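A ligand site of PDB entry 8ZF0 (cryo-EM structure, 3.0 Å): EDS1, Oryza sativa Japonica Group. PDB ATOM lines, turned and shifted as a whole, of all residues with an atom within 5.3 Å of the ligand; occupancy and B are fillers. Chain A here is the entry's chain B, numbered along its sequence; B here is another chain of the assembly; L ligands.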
ATOM      1  N   ARG A 455     -34.327 -19.356 -21.148  1.00  0.00           N
ATOM      2  CA  ARG A 455     -34.422 -20.149 -19.925  1.00  0.00           C
ATOM      3  C   ARG A 455     -33.496 -19.611 -18.841  1.00  0.00           C
ATOM      4  O   ARG A 455     -33.872 -19.551 -17.671  1.00  0.00           O
ATOM      5  CB  ARG A 455     -34.104 -21.618 -20.226  1.00  0.00           C
ATOM      6  CG  ARG A 455     -34.183 -22.524 -19.005  1.00  0.00           C
ATOM      7  CD  ARG A 455     -33.437 -23.828 -19.245  1.00  0.00           C
ATOM      8  NE  ARG A 455     -32.038 -23.600 -19.586  1.00  0.00           N
ATOM      9  CZ  ARG A 455     -31.014 -23.893 -18.797  1.00  0.00           C
ATOM     10  NH1 ARG A 455     -31.192 -24.434 -17.598  1.00  0.00           N
ATOM     11  NH2 ARG A 455     -29.778 -23.656 -19.218  1.00  0.00           N
ATOM     12  N   LEU A 456     -32.272 -19.222 -19.219  1.00  0.00           N
ATOM     13  CA  LEU A 456     -31.329 -18.676 -18.245  1.00  0.00           C
ATOM     14  C   LEU A 456     -31.835 -17.360 -17.661  1.00  0.00           C
ATOM     15  O   LEU A 456     -31.697 -17.119 -16.458  1.00  0.00           O
ATOM     16  CB  LEU A 456     -29.961 -18.496 -18.886  1.00  0.00           C
ATOM     17  CG  LEU A 456     -29.258 -19.783 -19.317  1.00  0.00           C
ATOM     18  CD1 LEU A 456     -28.040 -19.480 -20.164  1.00  0.00           C
ATOM     19  CD2 LEU A 456     -28.885 -20.619 -18.099  1.00  0.00           C
ATOM     20  N   ASP A 463     -35.247 -16.712  -9.296  1.00  0.00           N
ATOM     21  CA  ASP A 463     -34.391 -16.949  -8.142  1.00  0.00           C
ATOM     22  C   ASP A 463     -34.344 -15.739  -7.211  1.00  0.00           C
ATOM     23  O   ASP A 463     -34.240 -15.900  -5.993  1.00  0.00           O
ATOM     24  CB  ASP A 463     -32.983 -17.335  -8.583  1.00  0.00           C
ATOM     25  CG  ASP A 463     -32.829 -18.825  -8.797  1.00  0.00           C
ATOM     26  OD1 ASP A 463     -33.812 -19.560  -8.584  1.00  0.00           O
ATOM     27  OD2 ASP A 463     -31.722 -19.265  -9.179  1.00  0.00           O
ATOM     28  N   ARG A 470     -37.095 -15.997   1.208  1.00  0.00           N
ATOM     29  CA  ARG A 470     -36.484 -16.778   2.276  1.00  0.00           C
ATOM     30  C   ARG A 470     -36.133 -15.903   3.478  1.00  0.00           C
ATOM     31  O   ARG A 470     -36.284 -16.330   4.629  1.00  0.00           O
ATOM     32  CB  ARG A 470     -35.230 -17.489   1.759  1.00  0.00           C
ATOM     33  CG  ARG A 470     -35.522 -18.691   0.869  1.00  0.00           C
ATOM     34  CD  ARG A 470     -34.258 -19.191   0.190  1.00  0.00           C
ATOM     35  NE  ARG A 470     -33.156 -19.370   1.134  1.00  0.00           N
ATOM     36  CZ  ARG A 470     -31.995 -18.739   1.052  1.00  0.00           C
ATOM     37  NH1 ARG A 470     -31.738 -17.894   0.064  1.00  0.00           N
ATOM     38  NH2 ARG A 470     -31.062 -18.977   1.968  1.00  0.00           N
ATOM     39  N   ASP A 499     -35.420 -27.625 -18.366  1.00  0.00           N
ATOM     40  CA  ASP A 499     -34.402 -27.758 -17.335  1.00  0.00           C
ATOM     41  C   ASP A 499     -34.039 -29.218 -17.110  1.00  0.00           C
ATOM     42  O   ASP A 499     -32.872 -29.546 -16.841  1.00  0.00           O
ATOM     43  CB  ASP A 499     -34.880 -27.121 -16.028  1.00  0.00           C
ATOM     44  CG  ASP A 499     -34.263 -25.749 -15.798  1.00  0.00           C
ATOM     45  OD1 ASP A 499     -33.077 -25.563 -16.149  1.00  0.00           O
ATOM     46  OD2 ASP A 499     -34.965 -24.868 -15.268  1.00  0.00           O
ATOM     47  N   ILE A 500     -35.015 -30.126 -17.213  1.00  0.00           N
ATOM     48  CA  ILE A 500     -34.732 -31.555 -17.108  1.00  0.00           C
ATOM     49  C   ILE A 500     -33.824 -31.998 -18.251  1.00  0.00           C
ATOM     50  O   ILE A 500     -32.880 -32.765 -18.044  1.00  0.00           O
ATOM     51  CB  ILE A 500     -36.047 -32.352 -17.077  1.00  0.00           C
ATOM     52  CG1 ILE A 500     -36.798 -32.106 -15.765  1.00  0.00           C
ATOM     53  CG2 ILE A 500     -35.781 -33.840 -17.267  1.00  0.00           C
ATOM     54  CD1 ILE A 500     -38.164 -32.744 -15.714  1.00  0.00           C
ATOM     55  N   ASN A 502     -31.684 -30.153 -19.911  1.00  0.00           N
ATOM     56  CA  ASN A 502     -30.347 -29.611 -19.664  1.00  0.00           C
ATOM     57  C   ASN A 502     -29.596 -30.427 -18.626  1.00  0.00           C
ATOM     58  O   ASN A 502     -28.387 -30.628 -18.736  1.00  0.00           O
ATOM     59  CB  ASN A 502     -30.451 -28.149 -19.226  1.00  0.00           C
ATOM     60  CG  ASN A 502     -29.096 -27.466 -19.137  1.00  0.00           C
ATOM     61  OD1 ASN A 502     -28.402 -27.325 -20.145  1.00  0.00           O
ATOM     62  ND2 ASN A 502     -28.721 -27.046 -17.942  1.00  0.00           N
ATOM     63  N   TYR A 503     -30.305 -30.911 -17.599  1.00  0.00           N
ATOM     64  CA  TYR A 503     -29.666 -31.720 -16.563  1.00  0.00           C
ATOM     65  C   TYR A 503     -29.149 -33.034 -17.133  1.00  0.00           C
ATOM     66  O   TYR A 503     -28.050 -33.478 -16.776  1.00  0.00           O
ATOM     67  CB  TYR A 503     -30.648 -31.973 -15.428  1.00  0.00           C
ATOM     68  CG  TYR A 503     -30.017 -32.575 -14.192  1.00  0.00           C
ATOM     69  CD1 TYR A 503     -29.246 -31.794 -13.331  1.00  0.00           C
ATOM     70  CD2 TYR A 503     -30.191 -33.909 -13.873  1.00  0.00           C
ATOM     71  CE1 TYR A 503     -28.667 -32.339 -12.197  1.00  0.00           C
ATOM     72  CE2 TYR A 503     -29.615 -34.462 -12.750  1.00  0.00           C
ATOM     73  CZ  TYR A 503     -28.854 -33.670 -11.913  1.00  0.00           C
ATOM     74  OH  TYR A 503     -28.278 -34.223 -10.790  1.00  0.00           O
ATOM     75  N   LYS A 508     -25.229 -34.900 -15.920  1.00  0.00           N
ATOM     76  CA  LYS A 508     -25.164 -34.489 -14.525  1.00  0.00           C
ATOM     77  C   LYS A 508     -25.816 -35.487 -13.588  1.00  0.00           C
ATOM     78  O   LYS A 508     -25.744 -35.302 -12.361  1.00  0.00           O
ATOM     79  CB  LYS A 508     -25.810 -33.121 -14.351  1.00  0.00           C
ATOM     80  CG  LYS A 508     -25.176 -32.017 -15.183  1.00  0.00           C
ATOM     81  CD  LYS A 508     -25.624 -30.645 -14.719  1.00  0.00           C
ATOM     82  CE  LYS A 508     -24.669 -29.563 -15.213  1.00  0.00           C
ATOM     83  NZ  LYS A 508     -23.239 -29.948 -15.000  1.00  0.00           N
ATOM     84  N   ASP A 511     -22.807 -37.956 -11.738  1.00  0.00           N
ATOM     85  CA  ASP A 511     -21.853 -37.444 -10.760  1.00  0.00           C
ATOM     86  C   ASP A 511     -22.505 -36.827  -9.536  1.00  0.00           C
ATOM     87  O   ASP A 511     -21.833 -36.682  -8.504  1.00  0.00           O
ATOM     88  CB  ASP A 511     -20.924 -36.403 -11.396  1.00  0.00           C
ATOM     89  CG  ASP A 511     -21.654 -35.479 -12.359  1.00  0.00           C
ATOM     90  OD1 ASP A 511     -22.900 -35.537 -12.397  1.00  0.00           O
ATOM     91  OD2 ASP A 511     -20.979 -34.704 -13.062  1.00  0.00           O
ATOM     92  N   THR A 512     -23.792 -36.449  -9.602  1.00  0.00           N
ATOM     93  CA  THR A 512     -24.507 -35.883  -8.469  1.00  0.00           C
ATOM     94  C   THR A 512     -25.629 -36.780  -7.979  1.00  0.00           C
ATOM     95  O   THR A 512     -25.664 -37.111  -6.787  1.00  0.00           O
ATOM     96  CB  THR A 512     -25.080 -34.504  -8.848  1.00  0.00           C
ATOM     97  OG1 THR A 512     -24.005 -33.606  -9.153  1.00  0.00           O
ATOM     98  CG2 THR A 512     -25.903 -33.936  -7.705  1.00  0.00           C
ATOM     99  N   TYR A 515     -32.406 -36.506 -10.756  1.00  0.00           N
ATOM    100  CA  TYR A 515     -32.971 -35.158 -10.797  1.00  0.00           C
ATOM    101  C   TYR A 515     -34.020 -34.965  -9.708  1.00  0.00           C
ATOM    102  O   TYR A 515     -34.038 -33.938  -9.020  1.00  0.00           O
ATOM    103  CB  TYR A 515     -33.578 -34.885 -12.180  1.00  0.00           C
ATOM    104  CG  TYR A 515     -34.176 -33.506 -12.326  1.00  0.00           C
ATOM    105  CD1 TYR A 515     -33.395 -32.420 -12.684  1.00  0.00           C
ATOM    106  CD2 TYR A 515     -35.538 -33.287 -12.105  1.00  0.00           C
ATOM    107  CE1 TYR A 515     -33.941 -31.155 -12.821  1.00  0.00           C
ATOM    108  CE2 TYR A 515     -36.086 -32.036 -12.232  1.00  0.00           C
ATOM    109  CZ  TYR A 515     -35.293 -30.971 -12.596  1.00  0.00           C
ATOM    110  OH  TYR A 515     -35.832 -29.712 -12.731  1.00  0.00           O
ATOM    111  N   GLY A 519     -30.689 -33.212  -7.434  1.00  0.00           N
ATOM    112  CA  GLY A 519     -30.622 -31.932  -8.119  1.00  0.00           C
ATOM    113  C   GLY A 519     -31.933 -31.452  -8.707  1.00  0.00           C
ATOM    114  O   GLY A 519     -32.337 -31.911  -9.784  1.00  0.00           O
ATOM    115  N   ARG A 520     -32.584 -30.512  -8.028  1.00  0.00           N
ATOM    116  CA  ARG A 520     -33.813 -29.908  -8.523  1.00  0.00           C
ATOM    117  C   ARG A 520     -33.820 -28.447  -8.066  1.00  0.00           C
ATOM    118  O   ARG A 520     -33.553 -28.183  -6.878  1.00  0.00           O
ATOM    119  CB  ARG A 520     -35.067 -30.635  -8.027  1.00  0.00           C
ATOM    120  CG  ARG A 520     -36.353 -30.173  -8.691  1.00  0.00           C
ATOM    121  CD  ARG A 520     -37.585 -30.694  -7.966  1.00  0.00           C
ATOM    122  NE  ARG A 520     -38.812 -30.266  -8.612  1.00  0.00           N
ATOM    123  CZ  ARG A 520     -40.032 -30.542  -8.174  1.00  0.00           C
ATOM    124  NH1 ARG A 520     -40.220 -31.271  -7.076  1.00  0.00           N
ATOM    125  NH2 ARG A 520     -41.089 -30.095  -8.852  1.00  0.00           N
ATOM    126  N   PRO A 521     -34.097 -27.503  -8.957  1.00  0.00           N
ATOM    127  CA  PRO A 521     -34.110 -26.089  -8.552  1.00  0.00           C
ATOM    128  C   PRO A 521     -35.151 -25.825  -7.475  1.00  0.00           C
ATOM    129  O   PRO A 521     -36.236 -26.396  -7.477  1.00  0.00           O
ATOM    130  CB  PRO A 521     -34.442 -25.355  -9.859  1.00  0.00           C
ATOM    131  CG  PRO A 521     -34.016 -26.296 -10.940  1.00  0.00           C
ATOM    132  CD  PRO A 521     -34.291 -27.670 -10.409  1.00  0.00           C
ATOM    133  N   ARG A 522     -34.790 -24.933  -6.542  1.00  0.00           N
ATOM    134  CA  ARG A 522     -35.702 -24.602  -5.459  1.00  0.00           C
ATOM    135  C   ARG A 522     -36.895 -23.801  -5.951  1.00  0.00           C
ATOM    136  O   ARG A 522     -37.981 -23.856  -5.345  1.00  0.00           O
ATOM    137  CB  ARG A 522     -34.952 -23.822  -4.374  1.00  0.00           C
ATOM    138  CG  ARG A 522     -35.772 -23.511  -3.137  1.00  0.00           C
ATOM    139  CD  ARG A 522     -35.019 -22.597  -2.182  1.00  0.00           C
ATOM    140  NE  ARG A 522     -33.841 -23.238  -1.617  1.00  0.00           N
ATOM    141  CZ  ARG A 522     -33.867 -24.179  -0.682  1.00  0.00           C
ATOM    142  NH1 ARG A 522     -35.008 -24.605  -0.163  1.00  0.00           N
ATOM    143  NH2 ARG A 522     -32.722 -24.698  -0.246  1.00  0.00           N
ATOM    144  N   ARG A 523     -36.738 -23.062  -7.048  1.00  0.00           N
ATOM    145  CA  ARG A 523     -37.839 -22.259  -7.575  1.00  0.00           C
ATOM    146  C   ARG A 523     -39.003 -23.130  -8.019  1.00  0.00           C
ATOM    147  O   ARG A 523     -40.175 -22.788  -7.798  1.00  0.00           O
ATOM    148  CB  ARG A 523     -37.356 -21.384  -8.737  1.00  0.00           C
ATOM    149  CG  ARG A 523     -36.508 -22.118  -9.761  1.00  0.00           C
ATOM    150  CD  ARG A 523     -36.122 -21.212 -10.911  1.00  0.00           C
ATOM    151  NE  ARG A 523     -35.346 -21.905 -11.938  1.00  0.00           N
ATOM    152  CZ  ARG A 523     -34.076 -22.273 -11.794  1.00  0.00           C
ATOM    153  NH1 ARG A 523     -33.388 -22.013 -10.698  1.00  0.00           N
ATOM    154  NH2 ARG A 523     -33.479 -22.915 -12.793  1.00  0.00           N
ATOM    155  N   THR B 431     -24.610 -15.963 -17.788  1.00  0.00           N
ATOM    156  CA  THR B 431     -24.503 -17.377 -18.154  1.00  0.00           C
ATOM    157  C   THR B 431     -24.473 -17.676 -19.649  1.00  0.00           C
ATOM    158  O   THR B 431     -23.764 -18.610 -20.050  1.00  0.00           O
ATOM    159  CB  THR B 431     -25.647 -18.155 -17.477  1.00  0.00           C
ATOM    160  OG1 THR B 431     -25.691 -17.815 -16.082  1.00  0.00           O
ATOM    161  CG2 THR B 431     -25.420 -19.651 -17.605  1.00  0.00           C
ATOM    162  N   ARG B 434     -21.157 -18.517 -20.859  1.00  0.00           N
ATOM    163  CA  ARG B 434     -20.760 -19.889 -20.564  1.00  0.00           C
ATOM    164  C   ARG B 434     -21.405 -20.869 -21.527  1.00  0.00           C
ATOM    165  O   ARG B 434     -20.781 -21.870 -21.909  1.00  0.00           O
ATOM    166  CB  ARG B 434     -21.116 -20.234 -19.113  1.00  0.00           C
ATOM    167  CG  ARG B 434     -20.800 -21.666 -18.715  1.00  0.00           C
ATOM    168  CD  ARG B 434     -21.596 -22.096 -17.497  1.00  0.00           C
ATOM    169  NE  ARG B 434     -22.812 -22.804 -17.868  1.00  0.00           N
ATOM    170  CZ  ARG B 434     -23.909 -22.850 -17.130  1.00  0.00           C
ATOM    171  NH1 ARG B 434     -23.971 -22.243 -15.958  1.00  0.00           N
ATOM    172  NH2 ARG B 434     -24.975 -23.530 -17.571  1.00  0.00           N
ATOM    173  N   ARG B 496     -24.163 -21.858   0.174  1.00  0.00           N
ATOM    174  CA  ARG B 496     -25.379 -21.925  -0.617  1.00  0.00           C
ATOM    175  C   ARG B 496     -25.131 -22.812  -1.827  1.00  0.00           C
ATOM    176  O   ARG B 496     -24.122 -22.659  -2.522  1.00  0.00           O
ATOM    177  CB  ARG B 496     -25.830 -20.535  -1.064  1.00  0.00           C
ATOM    178  CG  ARG B 496     -26.122 -19.593   0.089  1.00  0.00           C
ATOM    179  CD  ARG B 496     -26.853 -18.347  -0.374  1.00  0.00           C
ATOM    180  NE  ARG B 496     -26.907 -17.333   0.670  1.00  0.00           N
ATOM    181  CZ  ARG B 496     -27.558 -16.186   0.568  1.00  0.00           C
ATOM    182  NH1 ARG B 496     -28.228 -15.871  -0.522  1.00  0.00           N
ATOM    183  NH2 ARG B 496     -27.531 -15.329   1.590  1.00  0.00           N
ATOM    184  N   ALA B 497     -26.054 -23.745  -2.070  1.00  0.00           N
ATOM    185  CA  ALA B 497     -25.852 -24.740  -3.123  1.00  0.00           C
ATOM    186  C   ALA B 497     -25.755 -24.108  -4.496  1.00  0.00           C
ATOM    187  O   ALA B 497     -24.918 -24.507  -5.316  1.00  0.00           O
ATOM    188  CB  ALA B 497     -26.978 -25.778  -3.079  1.00  0.00           C
ATOM    189  N   LYS B 498     -26.622 -23.130  -4.791  1.00  0.00           N
ATOM    190  CA  LYS B 498     -26.669 -22.549  -6.132  1.00  0.00           C
ATOM    191  C   LYS B 498     -25.325 -21.923  -6.504  1.00  0.00           C
ATOM    192  O   LYS B 498     -24.768 -22.211  -7.569  1.00  0.00           O
ATOM    193  CB  LYS B 498     -27.786 -21.515  -6.213  1.00  0.00           C
ATOM    194  CG  LYS B 498     -27.639 -20.577  -7.404  1.00  0.00           C
ATOM    195  CD  LYS B 498     -28.754 -19.540  -7.442  1.00  0.00           C
ATOM    196  CE  LYS B 498     -28.564 -18.587  -8.611  1.00  0.00           C
ATOM    197  NZ  LYS B 498     -29.713 -17.664  -8.780  1.00  0.00           N
ATOM    198  N   ASN B 501     -22.397 -24.575  -6.814  1.00  0.00           N
ATOM    199  CA  ASN B 501     -22.467 -25.435  -7.994  1.00  0.00           C
ATOM    200  C   ASN B 501     -22.257 -24.639  -9.276  1.00  0.00           C
ATOM    201  O   ASN B 501     -21.648 -25.134 -10.236  1.00  0.00           O
ATOM    202  CB  ASN B 501     -23.799 -26.204  -8.043  1.00  0.00           C
ATOM    203  CG  ASN B 501     -25.009 -25.302  -8.198  1.00  0.00           C
ATOM    204  OD1 ASN B 501     -25.102 -24.511  -9.133  1.00  0.00           O
ATOM    205  ND2 ASN B 501     -25.962 -25.461  -7.288  1.00  0.00           N
ATOM    206  N   ALA B 502     -22.739 -23.387  -9.320  1.00  0.00           N
ATOM    207  CA  ALA B 502     -22.454 -22.544 -10.477  1.00  0.00           C
ATOM    208  C   ALA B 502     -20.961 -22.274 -10.603  1.00  0.00           C
ATOM    209  O   ALA B 502     -20.397 -22.321 -11.706  1.00  0.00           O
ATOM    210  CB  ALA B 502     -23.229 -21.232 -10.371  1.00  0.00           C
ATOM    211  N   PHE B 505     -19.304 -25.465 -11.912  1.00  0.00           N
ATOM    212  CA  PHE B 505     -19.515 -25.597 -13.350  1.00  0.00           C
ATOM    213  C   PHE B 505     -18.595 -24.662 -14.131  1.00  0.00           C
ATOM    214  O   PHE B 505     -17.933 -25.071 -15.088  1.00  0.00           O
ATOM    215  CB  PHE B 505     -20.988 -25.334 -13.687  1.00  0.00           C
ATOM    216  CG  PHE B 505     -21.456 -26.000 -14.952  1.00  0.00           C
ATOM    217  CD1 PHE B 505     -20.563 -26.650 -15.789  1.00  0.00           C
ATOM    218  CD2 PHE B 505     -22.795 -25.957 -15.304  1.00  0.00           C
ATOM    219  CE1 PHE B 505     -21.002 -27.255 -16.954  1.00  0.00           C
ATOM    220  CE2 PHE B 505     -23.234 -26.561 -16.469  1.00  0.00           C
ATOM    221  CZ  PHE B 505     -22.344 -27.212 -17.296  1.00  0.00           C
HETATM  222  C1  LIG L   1     -28.388 -26.493  -9.933  1.00  0.00           C
HETATM  223  C2  LIG L   1     -30.020 -26.746 -10.027  1.00  0.00           C
HETATM  224  C3  LIG L   1     -30.568 -25.637  -9.176  1.00  0.00           C
HETATM  225  C4  LIG L   1     -29.372 -25.255  -8.246  1.00  0.00           C
HETATM  226  C5  LIG L   1     -29.627 -25.712  -6.927  1.00  0.00           C
HETATM  227  O1  LIG L   1     -30.475 -26.570 -11.424  1.00  0.00           O
HETATM  228  O2  LIG L   1     -29.604 -24.618  -6.082  1.00  0.00           O
HETATM  229  C6  LIG L   1     -24.454 -27.633 -11.499  1.00  0.00           C
HETATM  230  C7  LIG L   1     -30.597 -27.849 -12.093  1.00  0.00           C
HETATM  231  C8  LIG L   1     -29.073 -27.676 -14.066  1.00  0.00           C
HETATM  232  C9  LIG L   1     -27.855 -26.711 -14.080  1.00  0.00           C
HETATM  233  C10 LIG L   1     -30.159 -27.008 -14.322  1.00  0.00           C
HETATM  234  C11 LIG L   1     -31.339 -27.671 -13.377  1.00  0.00           C
HETATM  235  C12 LIG L   1     -26.489 -27.970 -10.489  1.00  0.00           C
HETATM  236  C13 LIG L   1     -26.204 -29.287 -10.325  1.00  0.00           C
HETATM  237  C14 LIG L   1     -24.968 -29.767 -10.793  1.00  0.00           C
HETATM  238  C15 LIG L   1     -28.153 -28.898  -9.514  1.00  0.00           C
HETATM  239  N1  LIG L   1     -24.142 -28.928 -11.359  1.00  0.00           N
HETATM  240  N2  LIG L   1     -25.603 -27.159 -11.068  1.00  0.00           N
HETATM  241  N3  LIG L   1     -24.609 -31.198 -10.644  1.00  0.00           N
HETATM  242  N4  LIG L   1     -27.245 -29.837  -9.729  1.00  0.00           N
HETATM  243  N5  LIG L   1     -27.706 -27.762  -9.975  1.00  0.00           N
HETATM  244  O3  LIG L   1     -31.814 -25.292  -4.998  1.00  0.00           O
HETATM  245  O4  LIG L   1     -31.063 -22.744  -1.741  1.00  0.00           O
HETATM  246  O5  LIG L   1     -29.203 -28.308 -12.630  1.00  0.00           O
HETATM  247  O6  LIG L   1     -31.802 -23.447  -6.555  1.00  0.00           O
HETATM  248  O7  LIG L   1     -30.290 -24.884  -2.518  1.00  0.00           O
HETATM  249  O8  LIG L   1     -30.924 -24.425 -10.059  1.00  0.00           O
HETATM  250  O9  LIG L   1     -27.762 -26.152 -15.378  1.00  0.00           O
HETATM  251  O10 LIG L   1     -28.765 -23.843 -14.739  1.00  0.00           O
HETATM  252  O11 LIG L   1     -26.318 -23.999 -14.980  1.00  0.00           O
HETATM  253  O12 LIG L   1     -27.797 -24.097 -17.009  1.00  0.00           O
HETATM  254  O13 LIG L   1     -30.513 -27.161 -15.697  1.00  0.00           O
HETATM  255  O14 LIG L   1     -31.741 -28.941 -13.933  1.00  0.00           O
HETATM  256  O15 LIG L   1     -30.792 -23.062  -4.291  1.00  0.00           O
HETATM  257  O16 LIG L   1     -28.793 -22.954  -2.618  1.00  0.00           O
HETATM  258  O17 LIG L   1     -28.133 -25.963  -8.789  1.00  0.00           O
HETATM  259  P1  LIG L   1     -27.658 -24.485 -15.522  1.00  0.00           P
HETATM  260  P2  LIG L   1     -31.031 -24.109  -5.485  1.00  0.00           P
HETATM  261  P3  LIG L   1     -30.222 -23.436  -2.759  1.00  0.00           P
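NH2 of Arg 523 lies within salt-bridge range of OD2 of Asp 499 (3.5 Å).
The side-chain amide nitrogen (ND2) of Asn 501 of chain B sits at hydrogen-bond distance from the backbone carbonyl oxygen (O) of Ala 497 of chain B, at 2.4 Å.
The side-chain carboxylate (OD1) of Asp 463 lies within salt-bridge range of the guanidinium group (NH1) of Arg 523, 3.3 Å away.
The side-chain amino group of Lys 498 of chain B lies within salt-bridge range of the side-chain carboxylate of Asp 463 (2.6 Å).
The side-chain amide oxygen of Asn 501 of chain B sits close to the backbone carbonyl oxygen of Lys 498 of chain B, 2.8 Å away.
The backbone carbonyl oxygen (O) of Lys 508 sits at hydrogen-bond distance from the side-chain hydroxyl (OH) of Tyr 503.
OD1 of Asp 499 is in salt-bridge range of NH1 of Arg 455, at 2.6 Å.
Residues that only touch the ligand: Tyr 515, Arg 523, Tyr 503, Pro 521, Arg 496 of chain B, Leu 456, Arg 520 and Lys 508.
17 residues have an atom within 4 Å of the ligand: Arg 455, Leu 456, Asp 499, Asn 502 of chain A, Tyr 503, Lys 508, Thr 512, Tyr 515, Arg 520, Pro 521, Arg 522, Arg 523, Arg 434 of chain B, Arg 496 of chain B, Ala 497 of chain B, Lys 498 of chain B and Asn 501 of chain B.
The side-chain hydroxyl (OG1) of Thr 512 is in hydrogen-bond range of a nitrogen (N3) of the ligand, at 2.9 Å.
O12 of the ligand lies within salt-bridge range of NH2 of Arg 455, 3.0 Å away.
The backbone NH of Ala 497 of chain B is in hydrogen-bond range of an oxygen (O16) of the ligand, at 2.9 Å.
O13 of the ligand lies within hydrogen-bond range of OD1 of Asp 499, at 3.1 Å.
The backbone carbonyl oxygen (O) of Asp 499 is in hydrogen-bond range of an oxygen (O14) of the ligand (3.2 Å).
An oxygen (O13) of the ligand sits at hydrogen-bond distance from the side-chain amide nitrogen (ND2) of Asn 502 of chain A (2.9 Å).
The backbone NH of Arg 522 sits at hydrogen-bond distance from an oxygen (O6) of the ligand, 3.3 Å away.
The side-chain amide nitrogen (ND2) of Asn 501 of chain B lies within hydrogen-bond range of an oxygen (O17) of the ligand (2.7 Å).
The guanidinium group (NE) of Arg 522 is in salt-bridge range of an oxygen (O4) of the ligand.
N of Lys 498 of chain B sits at hydrogen-bond distance from O16 of the ligand, at 3.1 Å.
The guanidinium group of Arg 434 of chain B is in salt-bridge range of an oxygen (O12) of the ligand, 2.9 Å away.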
